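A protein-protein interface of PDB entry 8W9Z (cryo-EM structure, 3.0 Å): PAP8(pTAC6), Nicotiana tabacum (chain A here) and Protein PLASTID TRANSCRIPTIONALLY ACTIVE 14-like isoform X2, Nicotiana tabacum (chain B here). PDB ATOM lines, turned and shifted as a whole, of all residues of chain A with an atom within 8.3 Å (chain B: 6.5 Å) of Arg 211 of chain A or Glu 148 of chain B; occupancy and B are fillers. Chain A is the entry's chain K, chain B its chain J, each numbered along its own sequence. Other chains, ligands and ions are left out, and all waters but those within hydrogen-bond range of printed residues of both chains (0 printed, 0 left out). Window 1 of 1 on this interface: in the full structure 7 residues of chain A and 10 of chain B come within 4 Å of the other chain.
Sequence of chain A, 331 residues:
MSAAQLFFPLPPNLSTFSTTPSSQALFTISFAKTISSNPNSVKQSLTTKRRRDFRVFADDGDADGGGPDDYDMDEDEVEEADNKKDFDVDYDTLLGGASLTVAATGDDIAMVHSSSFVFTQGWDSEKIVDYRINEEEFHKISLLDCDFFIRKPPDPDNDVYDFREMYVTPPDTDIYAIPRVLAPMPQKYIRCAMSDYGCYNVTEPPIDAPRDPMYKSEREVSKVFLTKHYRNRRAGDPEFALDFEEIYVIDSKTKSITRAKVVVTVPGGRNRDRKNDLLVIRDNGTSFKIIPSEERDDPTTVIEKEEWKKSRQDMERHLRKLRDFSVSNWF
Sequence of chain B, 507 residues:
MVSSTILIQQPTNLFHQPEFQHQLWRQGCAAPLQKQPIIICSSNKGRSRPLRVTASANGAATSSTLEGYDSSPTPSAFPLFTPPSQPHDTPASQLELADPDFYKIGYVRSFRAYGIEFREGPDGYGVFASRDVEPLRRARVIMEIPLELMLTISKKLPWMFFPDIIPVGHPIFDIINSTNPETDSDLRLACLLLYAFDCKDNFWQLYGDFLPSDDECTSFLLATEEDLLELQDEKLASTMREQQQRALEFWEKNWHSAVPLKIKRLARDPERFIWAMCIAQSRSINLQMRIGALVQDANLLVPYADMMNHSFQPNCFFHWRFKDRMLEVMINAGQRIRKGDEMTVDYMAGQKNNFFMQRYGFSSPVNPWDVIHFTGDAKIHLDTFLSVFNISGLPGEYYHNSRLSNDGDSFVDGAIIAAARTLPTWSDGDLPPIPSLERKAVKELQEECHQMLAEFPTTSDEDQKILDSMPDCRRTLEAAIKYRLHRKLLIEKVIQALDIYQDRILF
The guanidinium group (NH1) of Arg 211 of chain A sits at hydrogen-bond distance from the backbone carbonyl oxygen (O) of Asp 324 of chain B (2.9 Å). NH2 of Arg 325 of chain B sits at hydrogen-bond distance from O of Asp 208 of chain A (3.5 Å). The guanidinium group (NH2) of Arg 211 of chain A is in hydrogen-bond range of the side-chain sulfur (SD) of Met 326 of chain B (3.2 Å). The side-chain hydroxyl (OG) of Ser 110 of chain B sits at hydrogen-bond distance from the guanidinium group (NE) of Arg 211 of chain A (3.4 Å).
The backbone NH of Leu 147 of chain B lies within hydrogen-bond range of the backbone carbonyl oxygen of Arg 325 of chain B (3.0 Å).
Of the 8 printed residues of chain A, 4 touch a printed residue of chain B. Printed residues of chain A that touch a printed residue of chain B: Asp 208, Ala 209, Pro 210 and Arg 211. Along chain A the printed residues that touch a printed residue of chain B span positions 208 to 211. Hydrophobic or aromatic side chains of chain B that line the printed part of chain A: Pro 146 and Met 326. Among the printed residues, 10 pairs touch across the chains. Among the printed residues, no Asp or Glu carboxylate lies within 4 Å of a Lys or Arg side-chain nitrogen of the other chain.
Among the printed residues, merely in contact across the chains: Arg 211 of chain A with Glu 148 of chain B (3.3 Å), Pro 210 of chain A with Arg 325 of chain B (3.4 Å), Pro 210 of chain A with Asp 324 of chain B (3.4 Å), Ala 209 of chain A with Arg 325 of chain B (3.5 Å), Arg 211 of chain A with Pro 146 of chain B (3.7 Å) and Arg 211 of chain A with Arg 325 of chain B (3.9 Å).
Arg 211 of chain A touches six residues of chain B. Of chain A, only Arg 211 comes within 4 Å of Glu 148 of chain B. Printed residues of chain B within 4 Å of Asp 208 of chain A: Arg 325. Printed residues of chain B within 4 Å of Pro 210 of chain A: Asp 324 and Arg 325. Pro 163 of chain B touches none of the printed residues of chain A. The nearest residue of chain B that does not touch Arg 211 of chain A is Leu 147 of chain B (4.6 Å). The nearest printed residue of chain A that does not touch Met 326 of chain B is Pro 210 of chain A (6.6 Å).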
ATOM      1  N   ILE A 207      -8.919   4.836  18.508  1.00  0.00           N
ATOM      2  CA  ILE A 207      -7.795   5.488  17.844  1.00  0.00           C
ATOM      3  C   ILE A 207      -8.228   6.899  17.473  1.00  0.00           C
ATOM      4  O   ILE A 207      -9.013   7.095  16.538  1.00  0.00           O
ATOM      5  CB  ILE A 207      -7.332   4.706  16.607  1.00  0.00           C
ATOM      6  CG1 ILE A 207      -6.895   3.295  17.002  1.00  0.00           C
ATOM      7  CG2 ILE A 207      -6.199   5.439  15.910  1.00  0.00           C
ATOM      8  CD1 ILE A 207      -6.426   2.456  15.837  1.00  0.00           C
ATOM      9  N   ASP A 208      -7.716   7.886  18.207  1.00  0.00           N
ATOM     10  CA  ASP A 208      -7.967   9.299  17.947  1.00  0.00           C
ATOM     11  C   ASP A 208      -6.655  10.055  17.823  1.00  0.00           C
ATOM     12  O   ASP A 208      -6.502  11.168  18.334  1.00  0.00           O
ATOM     13  CB  ASP A 208      -8.845   9.910  19.035  1.00  0.00           C
ATOM     14  CG  ASP A 208     -10.313   9.589  18.847  1.00  0.00           C
ATOM     15  OD1 ASP A 208     -10.679   9.109  17.754  1.00  0.00           O
ATOM     16  OD2 ASP A 208     -11.100   9.813  19.791  1.00  0.00           O
ATOM     17  N   ALA A 209      -5.686   9.457  17.138  1.00  0.00           N
ATOM     18  CA  ALA A 209      -4.360  10.032  16.984  1.00  0.00           C
ATOM     19  C   ALA A 209      -3.722   9.430  15.741  1.00  0.00           C
ATOM     20  O   ALA A 209      -4.110   8.337  15.311  1.00  0.00           O
ATOM     21  CB  ALA A 209      -3.492   9.768  18.226  1.00  0.00           C
ATOM     22  N   PRO A 210      -2.747  10.116  15.137  1.00  0.00           N
ATOM     23  CA  PRO A 210      -2.101   9.555  13.941  1.00  0.00           C
ATOM     24  C   PRO A 210      -1.294   8.297  14.214  1.00  0.00           C
ATOM     25  O   PRO A 210      -1.084   7.510  13.283  1.00  0.00           O
ATOM     26  CB  PRO A 210      -1.201  10.699  13.455  1.00  0.00           C
ATOM     27  CG  PRO A 210      -0.967  11.536  14.667  1.00  0.00           C
ATOM     28  CD  PRO A 210      -2.240  11.462  15.454  1.00  0.00           C
ATOM     29  N   ARG A 211      -0.836   8.077  15.444  1.00  0.00           N
ATOM     30  CA  ARG A 211      -0.072   6.880  15.784  1.00  0.00           C
ATOM     31  C   ARG A 211      -0.538   6.310  17.118  1.00  0.00           C
ATOM     32  O   ARG A 211       0.271   5.896  17.955  1.00  0.00           O
ATOM     33  CB  ARG A 211       1.427   7.171  15.808  1.00  0.00           C
ATOM     34  CG  ARG A 211       1.830   8.311  16.729  1.00  0.00           C
ATOM     35  CD  ARG A 211       3.276   8.706  16.499  1.00  0.00           C
ATOM     36  NE  ARG A 211       3.488   9.182  15.137  1.00  0.00           N
ATOM     37  CZ  ARG A 211       3.283  10.435  14.748  1.00  0.00           C
ATOM     38  NH1 ARG A 211       2.864  11.339  15.622  1.00  0.00           N
ATOM     39  NH2 ARG A 211       3.499  10.785  13.488  1.00  0.00           N
ATOM     40  N   ASP A 212      -1.849   6.273  17.329  1.00  0.00           N
ATOM     41  CA  ASP A 212      -2.385   5.733  18.568  1.00  0.00           C
ATOM     42  C   ASP A 212      -2.153   4.224  18.627  1.00  0.00           C
ATOM     43  O   ASP A 212      -2.264   3.540  17.605  1.00  0.00           O
ATOM     44  CB  ASP A 212      -3.879   6.039  18.681  1.00  0.00           C
ATOM     45  CG  ASP A 212      -4.482   5.536  19.977  1.00  0.00           C
ATOM     46  OD1 ASP A 212      -4.248   6.168  21.029  1.00  0.00           O
ATOM     47  OD2 ASP A 212      -5.192   4.509  19.944  1.00  0.00           O
ATOM     48  N   PRO A 213      -1.813   3.683  19.797  1.00  0.00           N
ATOM     49  CA  PRO A 213      -1.607   2.234  19.905  1.00  0.00           C
ATOM     50  C   PRO A 213      -2.873   1.464  19.560  1.00  0.00           C
ATOM     51  O   PRO A 213      -3.974   1.813  19.992  1.00  0.00           O
ATOM     52  CB  PRO A 213      -1.213   2.041  21.373  1.00  0.00           C
ATOM     53  CG  PRO A 213      -0.660   3.362  21.791  1.00  0.00           C
ATOM     54  CD  PRO A 213      -1.459   4.386  21.041  1.00  0.00           C
ATOM     55  N   MET A 214      -2.705   0.404  18.769  1.00  0.00           N
ATOM     56  CA  MET A 214      -3.843  -0.379  18.306  1.00  0.00           C
ATOM     57  C   MET A 214      -4.361  -1.354  19.355  1.00  0.00           C
ATOM     58  O   MET A 214      -5.521  -1.771  19.271  1.00  0.00           O
ATOM     59  CB  MET A 214      -3.473  -1.143  17.034  1.00  0.00           C
ATOM     60  CG  MET A 214      -3.030  -0.255  15.886  1.00  0.00           C
ATOM     61  SD  MET A 214      -2.847  -1.165  14.341  1.00  0.00           S
ATOM     62  CE  MET A 214      -4.521  -1.752  14.102  1.00  0.00           C
ATOM     63  N   ARG B 109      10.002   4.333  18.877  1.00  0.00           N
ATOM     64  CA  ARG B 109       8.835   5.168  18.645  1.00  0.00           C
ATOM     65  C   ARG B 109       8.934   5.772  17.245  1.00  0.00           C
ATOM     66  O   ARG B 109       9.776   5.380  16.434  1.00  0.00           O
ATOM     67  CB  ARG B 109       8.717   6.241  19.725  1.00  0.00           C
ATOM     68  CG  ARG B 109       8.112   5.760  21.035  1.00  0.00           C
ATOM     69  CD  ARG B 109       9.139   5.087  21.926  1.00  0.00           C
ATOM     70  NE  ARG B 109       8.580   4.752  23.231  1.00  0.00           N
ATOM     71  CZ  ARG B 109       9.277   4.213  24.226  1.00  0.00           C
ATOM     72  NH1 ARG B 109      10.566   3.945  24.067  1.00  0.00           N
ATOM     73  NH2 ARG B 109       8.686   3.942  25.382  1.00  0.00           N
ATOM     74  N   SER B 110       8.072   6.740  16.943  1.00  0.00           N
ATOM     75  CA  SER B 110       8.056   7.366  15.623  1.00  0.00           C
ATOM     76  C   SER B 110       8.988   8.580  15.590  1.00  0.00           C
ATOM     77  O   SER B 110       8.589   9.706  15.301  1.00  0.00           O
ATOM     78  CB  SER B 110       6.631   7.747  15.238  1.00  0.00           C
ATOM     79  OG  SER B 110       6.595   8.361  13.961  1.00  0.00           O
ATOM     80  N   ILE B 145      10.020  14.677  15.820  1.00  0.00           N
ATOM     81  CA  ILE B 145       9.755  14.314  17.206  1.00  0.00           C
ATOM     82  C   ILE B 145       8.241  14.295  17.403  1.00  0.00           C
ATOM     83  O   ILE B 145       7.592  15.349  17.315  1.00  0.00           O
ATOM     84  CB  ILE B 145      10.433  15.289  18.177  1.00  0.00           C
ATOM     85  CG1 ILE B 145      11.866  15.561  17.718  1.00  0.00           C
ATOM     86  CG2 ILE B 145      10.420  14.728  19.587  1.00  0.00           C
ATOM     87  CD1 ILE B 145      12.533  16.714  18.422  1.00  0.00           C
ATOM     88  N   PRO B 146       7.636  13.141  17.667  1.00  0.00           N
ATOM     89  CA  PRO B 146       6.176  13.078  17.798  1.00  0.00           C
ATOM     90  C   PRO B 146       5.693  13.753  19.074  1.00  0.00           C
ATOM     91  O   PRO B 146       6.468  14.142  19.950  1.00  0.00           O
ATOM     92  CB  PRO B 146       5.883  11.576  17.812  1.00  0.00           C
ATOM     93  CG  PRO B 146       7.149  10.951  18.280  1.00  0.00           C
ATOM     94  CD  PRO B 146       8.258  11.810  17.751  1.00  0.00           C
ATOM     95  N   LEU B 147       4.368  13.887  19.165  1.00  0.00           N
ATOM     96  CA  LEU B 147       3.757  14.577  20.295  1.00  0.00           C
ATOM     97  C   LEU B 147       3.729  13.704  21.543  1.00  0.00           C
ATOM     98  O   LEU B 147       3.922  14.206  22.656  1.00  0.00           O
ATOM     99  CB  LEU B 147       2.340  15.022  19.933  1.00  0.00           C
ATOM    100  CG  LEU B 147       1.521  15.673  21.049  1.00  0.00           C
ATOM    101  CD1 LEU B 147       2.163  16.973  21.498  1.00  0.00           C
ATOM    102  CD2 LEU B 147       0.088  15.904  20.606  1.00  0.00           C
ATOM    103  N   GLU B 148       3.501  12.406  21.381  1.00  0.00           N
ATOM    104  CA  GLU B 148       3.390  11.482  22.508  1.00  0.00           C
ATOM    105  C   GLU B 148       4.706  11.257  23.232  1.00  0.00           C
ATOM    106  O   GLU B 148       4.750  10.421  24.144  1.00  0.00           O
ATOM    107  CB  GLU B 148       2.824  10.146  22.025  1.00  0.00           C
ATOM    108  CG  GLU B 148       3.623   9.504  20.903  1.00  0.00           C
ATOM    109  CD  GLU B 148       3.046   8.173  20.464  1.00  0.00           C
ATOM    110  OE1 GLU B 148       1.988   7.777  20.996  1.00  0.00           O
ATOM    111  OE2 GLU B 148       3.653   7.521  19.589  1.00  0.00           O
ATOM    112  N   LEU B 149       5.772  11.964  22.865  1.00  0.00           N
ATOM    113  CA  LEU B 149       7.071  11.818  23.502  1.00  0.00           C
ATOM    114  C   LEU B 149       7.475  13.034  24.325  1.00  0.00           C
ATOM    115  O   LEU B 149       8.585  13.052  24.866  1.00  0.00           O
ATOM    116  CB  LEU B 149       8.148  11.536  22.449  1.00  0.00           C
ATOM    117  CG  LEU B 149       8.467  10.082  22.098  1.00  0.00           C
ATOM    118  CD1 LEU B 149       7.235   9.342  21.608  1.00  0.00           C
ATOM    119  CD2 LEU B 149       9.573  10.027  21.058  1.00  0.00           C
ATOM    120  N   MET B 150       6.613  14.041  24.443  1.00  0.00           N
ATOM    121  CA  MET B 150       6.972  15.274  25.123  1.00  0.00           C
ATOM    122  C   MET B 150       5.817  15.749  25.994  1.00  0.00           C
ATOM    123  O   MET B 150       4.668  15.337  25.823  1.00  0.00           O
ATOM    124  CB  MET B 150       7.369  16.367  24.124  1.00  0.00           C
ATOM    125  CG  MET B 150       6.390  16.566  22.982  1.00  0.00           C
ATOM    126  SD  MET B 150       7.036  17.705  21.745  1.00  0.00           S
ATOM    127  CE  MET B 150       5.717  17.684  20.538  1.00  0.00           C
ATOM    128  N   PRO B 163      -0.847  15.767  25.678  1.00  0.00           N
ATOM    129  CA  PRO B 163      -0.544  14.376  26.042  1.00  0.00           C
ATOM    130  C   PRO B 163      -1.113  14.079  27.421  1.00  0.00           C
ATOM    131  O   PRO B 163      -0.527  14.444  28.446  1.00  0.00           O
ATOM    132  CB  PRO B 163       0.990  14.339  26.026  1.00  0.00           C
ATOM    133  CG  PRO B 163       1.396  15.727  26.332  1.00  0.00           C
ATOM    134  CD  PRO B 163       0.362  16.611  25.703  1.00  0.00           C
ATOM    135  N   ASN B 202       6.317   5.270  30.256  1.00  0.00           N
ATOM    136  CA  ASN B 202       6.536   6.649  29.852  1.00  0.00           C
ATOM    137  C   ASN B 202       7.946   6.796  29.296  1.00  0.00           C
ATOM    138  O   ASN B 202       8.880   6.141  29.767  1.00  0.00           O
ATOM    139  CB  ASN B 202       6.330   7.609  31.027  1.00  0.00           C
ATOM    140  CG  ASN B 202       6.113   9.041  30.581  1.00  0.00           C
ATOM    141  OD1 ASN B 202       6.536   9.438  29.496  1.00  0.00           O
ATOM    142  ND2 ASN B 202       5.449   9.825  31.421  1.00  0.00           N
ATOM    143  N   PHE B 203       8.092   7.660  28.290  1.00  0.00           N
ATOM    144  CA  PHE B 203       9.390   7.826  27.646  1.00  0.00           C
ATOM    145  C   PHE B 203      10.394   8.513  28.560  1.00  0.00           C
ATOM    146  O   PHE B 203      11.603   8.301  28.418  1.00  0.00           O
ATOM    147  CB  PHE B 203       9.233   8.614  26.346  1.00  0.00           C
ATOM    148  CG  PHE B 203      10.516   8.798  25.589  1.00  0.00           C
ATOM    149  CD1 PHE B 203      10.991   7.801  24.759  1.00  0.00           C
ATOM    150  CD2 PHE B 203      11.241   9.969  25.703  1.00  0.00           C
ATOM    151  CE1 PHE B 203      12.169   7.967  24.062  1.00  0.00           C
ATOM    152  CE2 PHE B 203      12.418  10.141  25.008  1.00  0.00           C
ATOM    153  CZ  PHE B 203      12.884   9.138  24.186  1.00  0.00           C
ATOM    154  N   ASP B 324       0.560  15.403  11.322  1.00  0.00           N
ATOM    155  CA  ASP B 324       1.037  14.222  12.025  1.00  0.00           C
ATOM    156  C   ASP B 324       1.342  14.483  13.492  1.00  0.00           C
ATOM    157  O   ASP B 324       1.753  13.552  14.194  1.00  0.00           O
ATOM    158  CB  ASP B 324       2.290  13.662  11.340  1.00  0.00           C
ATOM    159  CG  ASP B 324       2.034  13.246   9.907  1.00  0.00           C
ATOM    160  OD1 ASP B 324       0.889  12.856   9.594  1.00  0.00           O
ATOM    161  OD2 ASP B 324       2.979  13.308   9.094  1.00  0.00           O
ATOM    162  N   ARG B 325       1.149  15.712  13.969  1.00  0.00           N
ATOM    163  CA  ARG B 325       1.453  16.090  15.348  1.00  0.00           C
ATOM    164  C   ARG B 325       2.901  15.758  15.700  1.00  0.00           C
ATOM    165  O   ARG B 325       3.190  15.066  16.678  1.00  0.00           O
ATOM    166  CB  ARG B 325       0.477  15.435  16.326  1.00  0.00           C
ATOM    167  CG  ARG B 325      -0.935  15.992  16.249  1.00  0.00           C
ATOM    168  CD  ARG B 325      -1.768  15.560  17.443  1.00  0.00           C
ATOM    169  NE  ARG B 325      -2.653  14.444  17.130  1.00  0.00           N
ATOM    170  CZ  ARG B 325      -3.936  14.578  16.814  1.00  0.00           C
ATOM    171  NH1 ARG B 325      -4.486  15.784  16.768  1.00  0.00           N
ATOM    172  NH2 ARG B 325      -4.672  13.509  16.544  1.00  0.00           N
ATOM    173  N   MET B 326       3.821  16.267  14.882  1.00  0.00           N
ATOM    174  CA  MET B 326       5.248  16.072  15.083  1.00  0.00           C
ATOM    175  C   MET B 326       5.969  17.403  14.946  1.00  0.00           C
ATOM    176  O   MET B 326       5.659  18.198  14.055  1.00  0.00           O
ATOM    177  CB  MET B 326       5.824  15.066  14.079  1.00  0.00           C
ATOM    178  CG  MET B 326       5.300  13.650  14.240  1.00  0.00           C
ATOM    179  SD  MET B 326       6.220  12.453  13.254  1.00  0.00           S
ATOM    180  CE  MET B 326       5.969  13.105  11.607  1.00  0.00           C
